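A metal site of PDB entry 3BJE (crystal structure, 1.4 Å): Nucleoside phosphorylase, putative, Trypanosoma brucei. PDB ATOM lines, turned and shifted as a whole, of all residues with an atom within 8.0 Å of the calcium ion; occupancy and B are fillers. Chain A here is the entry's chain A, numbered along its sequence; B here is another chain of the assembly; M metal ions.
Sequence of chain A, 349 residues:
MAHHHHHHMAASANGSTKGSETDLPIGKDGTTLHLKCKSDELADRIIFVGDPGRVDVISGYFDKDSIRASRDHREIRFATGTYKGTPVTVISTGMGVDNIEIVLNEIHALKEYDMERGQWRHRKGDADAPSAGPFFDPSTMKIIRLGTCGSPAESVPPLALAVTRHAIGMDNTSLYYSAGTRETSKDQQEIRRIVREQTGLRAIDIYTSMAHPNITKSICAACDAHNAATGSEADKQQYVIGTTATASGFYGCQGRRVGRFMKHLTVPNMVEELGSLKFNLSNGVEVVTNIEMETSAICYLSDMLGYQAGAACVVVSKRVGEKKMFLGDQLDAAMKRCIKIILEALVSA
OE2 of Glu 75 of chain A sits at hydrogen-bond distance from N of Met 95 of chain B (2.9 Å). N of Met 95 of chain A lies within hydrogen-bond range of OE2 of Glu 75 of chain B, at 3.0 Å. The side-chain amide nitrogen (ND2) of Asn 99 of chain B lies within hydrogen-bond range of the side-chain carboxylate (OE2) of Glu 75 of chain B (3.0 Å). The backbone carbonyl oxygen (O) of Thr 93 of chain B lies within hydrogen-bond range of the side-chain amide nitrogen (ND2) of Asn 99 of chain B (2.8 Å). The side-chain amide nitrogen (ND2) of Asn 99 of chain A sits at hydrogen-bond distance from the side-chain carboxylate (OE2) of Glu 75 of chain A (3.0 Å). The side-chain amide nitrogen (ND2) of Asn 99 of chain A sits at hydrogen-bond distance from the backbone carbonyl oxygen (O) of Thr 93 of chain A.
The calcium ion is bound by O of Met 95 of chain B (2.4 Å), O of Met 95 of chain A (2.4 Å), OD1 of Asn 99 of chain B (2.4 Å), OD1 of Asn 99 of chain A (2.4 Å), OD1 of Asp 98 of chain A (2.4 Å), OD1 of Asp 98 of chain B (2.4 Å), OD2 of Asp 98 of chain B (2.7 Å) and OD2 of Asp 98 of chain A (2.8 Å).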
ATOM      1  N   GLU A  75       0.088 -28.342  24.358  1.00  0.00           N
ATOM      2  CA  GLU A  75      -0.668 -28.458  25.617  1.00  0.00           C
ATOM      3  C   GLU A  75      -1.320 -29.866  25.765  1.00  0.00           C
ATOM      4  O   GLU A  75      -2.028 -30.134  26.733  1.00  0.00           O
ATOM      5  CB  GLU A  75      -1.679 -27.296  25.769  1.00  0.00           C
ATOM      6  CG  GLU A  75      -2.730 -27.018  24.638  1.00  0.00           C
ATOM      7  CD  GLU A  75      -2.393 -25.755  23.836  1.00  0.00           C
ATOM      8  OE1 GLU A  75      -1.278 -25.876  23.249  1.00  0.00           O
ATOM      9  OE2 GLU A  75      -3.161 -24.678  23.822  1.00  0.00           O
ATOM     10  N   THR A  93      -6.419 -31.032  27.045  1.00  0.00           N
ATOM     11  CA  THR A  93      -6.798 -30.336  25.845  1.00  0.00           C
ATOM     12  C   THR A  93      -6.223 -28.938  25.743  1.00  0.00           C
ATOM     13  O   THR A  93      -6.241 -28.347  24.664  1.00  0.00           O
ATOM     14  CB  THR A  93      -8.326 -30.222  25.779  1.00  0.00           C
ATOM     15  OG1 THR A  93      -8.787 -29.417  26.868  1.00  0.00           O
ATOM     16  CG2 THR A  93      -8.997 -31.597  25.853  1.00  0.00           C
ATOM     17  N   GLY A  94      -5.711 -28.416  26.847  1.00  0.00           N
ATOM     18  CA  GLY A  94      -5.428 -26.991  26.937  1.00  0.00           C
ATOM     19  C   GLY A  94      -6.742 -26.237  27.019  1.00  0.00           C
ATOM     20  O   GLY A  94      -7.810 -26.835  27.132  1.00  0.00           O
ATOM     21  N   MET A  95      -6.668 -24.914  26.911  1.00  0.00           N
ATOM     22  CA  MET A  95      -7.826 -24.080  27.199  1.00  0.00           C
ATOM     23  C   MET A  95      -8.653 -23.810  25.962  1.00  0.00           C
ATOM     24  O   MET A  95      -8.101 -23.451  24.926  1.00  0.00           O
ATOM     25  CB  MET A  95      -7.370 -22.775  27.822  1.00  0.00           C
ATOM     26  CG  MET A  95      -6.567 -22.985  29.059  1.00  0.00           C
ATOM     27  SD  MET A  95      -6.150 -21.470  29.932  1.00  0.00           S
ATOM     28  CE  MET A  95      -4.855 -20.843  28.886  1.00  0.00           C
ATOM     29  N   GLY A  96      -9.965 -23.990  26.071  1.00  0.00           N
ATOM     30  CA  GLY A  96     -10.879 -23.487  25.070  1.00  0.00           C
ATOM     31  C   GLY A  96     -11.580 -24.455  24.125  1.00  0.00           C
ATOM     32  O   GLY A  96     -11.134 -25.578  23.905  1.00  0.00           O
ATOM     33  N   VAL A  97     -12.700 -23.978  23.596  1.00  0.00           N
ATOM     34  CA  VAL A  97     -13.517 -24.755  22.659  1.00  0.00           C
ATOM     35  C   VAL A  97     -12.825 -24.998  21.320  1.00  0.00           C
ATOM     36  O   VAL A  97     -13.111 -25.977  20.632  1.00  0.00           O
ATOM     37  CB  VAL A  97     -14.903 -24.088  22.410  1.00  0.00           C
ATOM     38  CG1 VAL A  97     -15.811 -24.221  23.656  1.00  0.00           C
ATOM     39  CG2 VAL A  97     -14.747 -22.629  21.945  1.00  0.00           C
ATOM     40  N   ASP A  98     -11.907 -24.108  20.981  1.00  0.00           N
ATOM     41  CA  ASP A  98     -11.094 -24.280  19.794  1.00  0.00           C
ATOM     42  C   ASP A  98     -10.162 -25.485  19.962  1.00  0.00           C
ATOM     43  O   ASP A  98     -10.014 -26.293  19.046  1.00  0.00           O
ATOM     44  CB  ASP A  98     -10.305 -23.006  19.487  1.00  0.00           C
ATOM     45  CG  ASP A  98      -9.380 -22.584  20.602  1.00  0.00           C
ATOM     46  OD1 ASP A  98      -9.698 -22.727  21.801  1.00  0.00           O
ATOM     47  OD2 ASP A  98      -8.325 -22.021  20.303  1.00  0.00           O
ATOM     48  N   ASN A  99      -9.578 -25.607  21.153  1.00  0.00           N
ATOM     49  CA  ASN A  99      -8.745 -26.775  21.498  1.00  0.00           C
ATOM     50  C   ASN A  99      -9.569 -28.056  21.491  1.00  0.00           C
ATOM     51  O   ASN A  99      -9.116 -29.126  21.066  1.00  0.00           O
ATOM     52  CB  ASN A  99      -8.088 -26.563  22.860  1.00  0.00           C
ATOM     53  CG  ASN A  99      -6.987 -25.515  22.823  1.00  0.00           C
ATOM     54  OD1 ASN A  99      -7.191 -24.377  22.331  1.00  0.00           O
ATOM     55  ND2 ASN A  99      -5.825 -25.878  23.341  1.00  0.00           N
ATOM     56  N   ILE A 100     -10.807 -27.951  21.988  1.00  0.00           N
ATOM     57  CA  ILE A 100     -11.745 -29.072  21.950  1.00  0.00           C
ATOM     58  C   ILE A 100     -12.010 -29.514  20.516  1.00  0.00           C
ATOM     59  O   ILE A 100     -12.015 -30.708  20.203  1.00  0.00           O
ATOM     60  CB  ILE A 100     -13.081 -28.734  22.704  1.00  0.00           C
ATOM     61  CG1 ILE A 100     -12.875 -28.516  24.214  1.00  0.00           C
ATOM     62  CG2 ILE A 100     -14.114 -29.838  22.447  1.00  0.00           C
ATOM     63  CD1 ILE A 100     -12.140 -29.631  24.953  1.00  0.00           C
ATOM     64  N   ILE A 102     -10.134 -29.218  17.967  1.00  0.00           N
ATOM     65  CA  ILE A 102      -8.958 -29.946  17.514  1.00  0.00           C
ATOM     66  C   ILE A 102      -8.968 -31.387  18.034  1.00  0.00           C
ATOM     67  O   ILE A 102      -8.862 -32.357  17.277  1.00  0.00           O
ATOM     68  CB  ILE A 102      -7.690 -29.228  17.971  1.00  0.00           C
ATOM     69  CG1 ILE A 102      -7.491 -27.956  17.144  1.00  0.00           C
ATOM     70  CG2 ILE A 102      -6.464 -30.158  17.804  1.00  0.00           C
ATOM     71  CD1 ILE A 102      -6.413 -27.028  17.672  1.00  0.00           C
ATOM     72  N   SER A 248     -15.493 -17.722  25.196  1.00  0.00           N
ATOM     73  CA  SER A 248     -14.364 -17.690  24.241  1.00  0.00           C
ATOM     74  C   SER A 248     -13.173 -16.857  24.769  1.00  0.00           C
ATOM     75  O   SER A 248     -12.400 -16.277  24.016  1.00  0.00           O
ATOM     76  CB  SER A 248     -14.834 -17.192  22.888  1.00  0.00           C
ATOM     77  OG  SER A 248     -15.517 -15.939  22.981  1.00  0.00           O
ATOM     78  N   MET A 293     -14.683 -22.722  29.845  1.00  0.00           N
ATOM     79  CA  MET A 293     -14.213 -22.450  28.477  1.00  0.00           C
ATOM     80  C   MET A 293     -14.248 -23.605  27.467  1.00  0.00           C
ATOM     81  O   MET A 293     -13.792 -23.426  26.337  1.00  0.00           O
ATOM     82  CB  MET A 293     -12.791 -21.863  28.538  1.00  0.00           C
ATOM     83  CG  MET A 293     -12.736 -20.526  29.243  1.00  0.00           C
ATOM     84  SD  MET A 293     -11.098 -19.797  29.381  1.00  0.00           S
ATOM     85  CE  MET A 293     -10.686 -19.532  27.619  1.00  0.00           C
ATOM     86  N   GLU A 294     -14.791 -24.772  27.837  1.00  0.00           N
ATOM     87  CA  GLU A 294     -14.770 -25.955  26.946  1.00  0.00           C
ATOM     88  C   GLU A 294     -16.076 -26.705  26.705  1.00  0.00           C
ATOM     89  O   GLU A 294     -16.227 -27.373  25.687  1.00  0.00           O
ATOM     90  CB  GLU A 294     -13.729 -26.963  27.470  1.00  0.00           C
ATOM     91  CG  GLU A 294     -12.277 -26.468  27.356  1.00  0.00           C
ATOM     92  CD  GLU A 294     -11.741 -25.809  28.628  1.00  0.00           C
ATOM     93  OE1 GLU A 294     -12.142 -26.186  29.739  1.00  0.00           O
ATOM     94  OE2 GLU A 294     -10.887 -24.877  28.534  1.00  0.00           O
ATOM     95  N   GLU B  75      -0.037 -24.194  29.295  1.00  0.00           N
ATOM     96  CA  GLU B  75       0.638 -24.008  28.018  1.00  0.00           C
ATOM     97  C   GLU B  75       1.442 -22.681  27.977  1.00  0.00           C
ATOM     98  O   GLU B  75       2.023 -22.339  26.940  1.00  0.00           O
ATOM     99  CB  GLU B  75      -0.387 -24.128  26.867  1.00  0.00           C
ATOM    100  CG  GLU B  75      -1.586 -23.142  26.838  1.00  0.00           C
ATOM    101  CD  GLU B  75      -2.933 -23.772  27.253  1.00  0.00           C
ATOM    102  OE1 GLU B  75      -2.940 -24.172  28.435  1.00  0.00           O
ATOM    103  OE2 GLU B  75      -3.932 -23.868  26.429  1.00  0.00           O
ATOM    104  N   THR B  93       1.532 -18.797  24.113  1.00  0.00           N
ATOM    105  CA  THR B  93       0.145 -18.535  24.453  1.00  0.00           C
ATOM    106  C   THR B  93      -0.714 -19.776  24.423  1.00  0.00           C
ATOM    107  O   THR B  93      -1.819 -19.778  24.995  1.00  0.00           O
ATOM    108  CB  THR B  93      -0.460 -17.535  23.454  1.00  0.00           C
ATOM    109  OG1 THR B  93      -0.347 -18.029  22.117  1.00  0.00           O
ATOM    110  CG2 THR B  93       0.268 -16.192  23.558  1.00  0.00           C
ATOM    111  N   GLY B  94      -0.191 -20.852  23.825  1.00  0.00           N
ATOM    112  CA  GLY B  94      -1.055 -21.980  23.480  1.00  0.00           C
ATOM    113  C   GLY B  94      -1.915 -21.572  22.283  1.00  0.00           C
ATOM    114  O   GLY B  94      -1.701 -20.531  21.676  1.00  0.00           O
ATOM    115  N   MET B  95      -2.907 -22.392  21.975  1.00  0.00           N
ATOM    116  CA  MET B  95      -3.683 -22.203  20.749  1.00  0.00           C
ATOM    117  C   MET B  95      -4.917 -21.361  21.006  1.00  0.00           C
ATOM    118  O   MET B  95      -5.629 -21.575  21.968  1.00  0.00           O
ATOM    119  CB  MET B  95      -4.101 -23.565  20.203  1.00  0.00           C
ATOM    120  CG  MET B  95      -2.894 -24.448  19.966  1.00  0.00           C
ATOM    121  SD  MET B  95      -3.192 -25.988  19.102  1.00  0.00           S
ATOM    122  CE  MET B  95      -3.998 -26.929  20.385  1.00  0.00           C
ATOM    123  N   GLY B  96      -5.104 -20.373  20.152  1.00  0.00           N
ATOM    124  CA  GLY B  96      -6.398 -19.702  19.985  1.00  0.00           C
ATOM    125  C   GLY B  96      -6.515 -18.281  20.490  1.00  0.00           C
ATOM    126  O   GLY B  96      -5.736 -17.806  21.332  1.00  0.00           O
ATOM    127  N   VAL B  97      -7.537 -17.611  19.971  1.00  0.00           N
ATOM    128  CA  VAL B  97      -7.827 -16.233  20.362  1.00  0.00           C
ATOM    129  C   VAL B  97      -8.299 -16.087  21.821  1.00  0.00           C
ATOM    130  O   VAL B  97      -8.131 -15.039  22.455  1.00  0.00           O
ATOM    131  CB  VAL B  97      -8.845 -15.604  19.403  1.00  0.00           C
ATOM    132  CG1 VAL B  97      -8.176 -15.377  18.026  1.00  0.00           C
ATOM    133  CG2 VAL B  97     -10.081 -16.478  19.252  1.00  0.00           C
ATOM    134  N   ASP B  98      -8.889 -17.152  22.337  1.00  0.00           N
ATOM    135  CA  ASP B  98      -9.245 -17.228  23.747  1.00  0.00           C
ATOM    136  C   ASP B  98      -8.015 -17.185  24.625  1.00  0.00           C
ATOM    137  O   ASP B  98      -7.987 -16.452  25.625  1.00  0.00           O
ATOM    138  CB  ASP B  98     -10.090 -18.475  24.048  1.00  0.00           C
ATOM    139  CG  ASP B  98      -9.376 -19.785  23.716  1.00  0.00           C
ATOM    140  OD1 ASP B  98      -8.599 -19.851  22.754  1.00  0.00           O
ATOM    141  OD2 ASP B  98      -9.626 -20.791  24.405  1.00  0.00           O
ATOM    142  N   ASN B  99      -6.979 -17.931  24.229  1.00  0.00           N
ATOM    143  CA  ASN B  99      -5.697 -17.888  24.918  1.00  0.00           C
ATOM    144  C   ASN B  99      -5.046 -16.516  24.833  1.00  0.00           C
ATOM    145  O   ASN B  99      -4.443 -16.042  25.800  1.00  0.00           O
ATOM    146  CB  ASN B  99      -4.776 -18.965  24.369  1.00  0.00           C
ATOM    147  CG  ASN B  99      -5.212 -20.358  24.770  1.00  0.00           C
ATOM    148  OD1 ASN B  99      -6.364 -20.755  24.539  1.00  0.00           O
ATOM    149  ND2 ASN B  99      -4.284 -21.131  25.325  1.00  0.00           N
ATOM    150  N   ILE B 100      -5.172 -15.883  23.671  1.00  0.00           N
ATOM    151  CA  ILE B 100      -4.673 -14.519  23.501  1.00  0.00           C
ATOM    152  C   ILE B 100      -5.376 -13.543  24.454  1.00  0.00           C
ATOM    153  O   ILE B 100      -4.766 -12.666  25.058  1.00  0.00           O
ATOM    154  CB  ILE B 100      -4.872 -14.028  22.058  1.00  0.00           C
ATOM    155  CG1 ILE B 100      -4.021 -14.860  21.075  1.00  0.00           C
ATOM    156  CG2 ILE B 100      -4.558 -12.539  21.925  1.00  0.00           C
ATOM    157  CD1 ILE B 100      -2.538 -14.961  21.469  1.00  0.00           C
ATOM    158  N   ILE B 102      -6.681 -14.180  27.304  1.00  0.00           N
ATOM    159  CA  ILE B 102      -6.089 -14.379  28.635  1.00  0.00           C
ATOM    160  C   ILE B 102      -4.744 -13.654  28.768  1.00  0.00           C
ATOM    161  O   ILE B 102      -4.535 -12.884  29.715  1.00  0.00           O
ATOM    162  CB  ILE B 102      -5.928 -15.890  28.933  1.00  0.00           C
ATOM    163  CG1 ILE B 102      -7.317 -16.521  29.177  1.00  0.00           C
ATOM    164  CG2 ILE B 102      -4.979 -16.113  30.119  1.00  0.00           C
ATOM    165  CD1 ILE B 102      -7.336 -18.059  29.162  1.00  0.00           C
ATOM    166  N   SER B 248     -11.673 -20.154  14.976  1.00  0.00           N
ATOM    167  CA  SER B 248     -11.964 -20.600  16.321  1.00  0.00           C
ATOM    168  C   SER B 248     -11.822 -22.140  16.396  1.00  0.00           C
ATOM    169  O   SER B 248     -12.504 -22.805  17.164  1.00  0.00           O
ATOM    170  CB  SER B 248     -13.374 -20.142  16.751  1.00  0.00           C
ATOM    171  OG  SER B 248     -14.315 -20.482  15.750  1.00  0.00           O
ATOM    172  N   MET B 293      -4.885 -19.203  14.060  1.00  0.00           N
ATOM    173  CA  MET B 293      -5.823 -19.221  15.212  1.00  0.00           C
ATOM    174  C   MET B 293      -5.683 -18.107  16.238  1.00  0.00           C
ATOM    175  O   MET B 293      -6.418 -18.108  17.215  1.00  0.00           O
ATOM    176  CB  MET B 293      -5.773 -20.609  15.878  1.00  0.00           C
ATOM    177  CG  MET B 293      -6.239 -21.738  14.951  1.00  0.00           C
ATOM    178  SD  MET B 293      -6.151 -23.359  15.727  1.00  0.00           S
ATOM    179  CE  MET B 293      -7.365 -23.167  17.081  1.00  0.00           C
ATOM    180  N   GLU B 294      -4.774 -17.149  16.033  1.00  0.00           N
ATOM    181  CA  GLU B 294      -4.542 -16.120  17.074  1.00  0.00           C
ATOM    182  C   GLU B 294      -4.592 -14.656  16.650  1.00  0.00           C
ATOM    183  O   GLU B 294      -4.814 -13.787  17.463  1.00  0.00           O
ATOM    184  CB  GLU B 294      -3.173 -16.377  17.731  1.00  0.00           C
ATOM    185  CG  GLU B 294      -3.105 -17.637  18.615  1.00  0.00           C
ATOM    186  CD  GLU B 294      -2.671 -18.880  17.860  1.00  0.00           C
ATOM    187  OE1 GLU B 294      -1.753 -18.780  17.047  1.00  0.00           O
ATOM    188  OE2 GLU B 294      -3.217 -19.984  18.129  1.00  0.00           O
HETATM  189 CA    CA M   1      -7.682 -22.096  23.002  1.00  0.00          CA
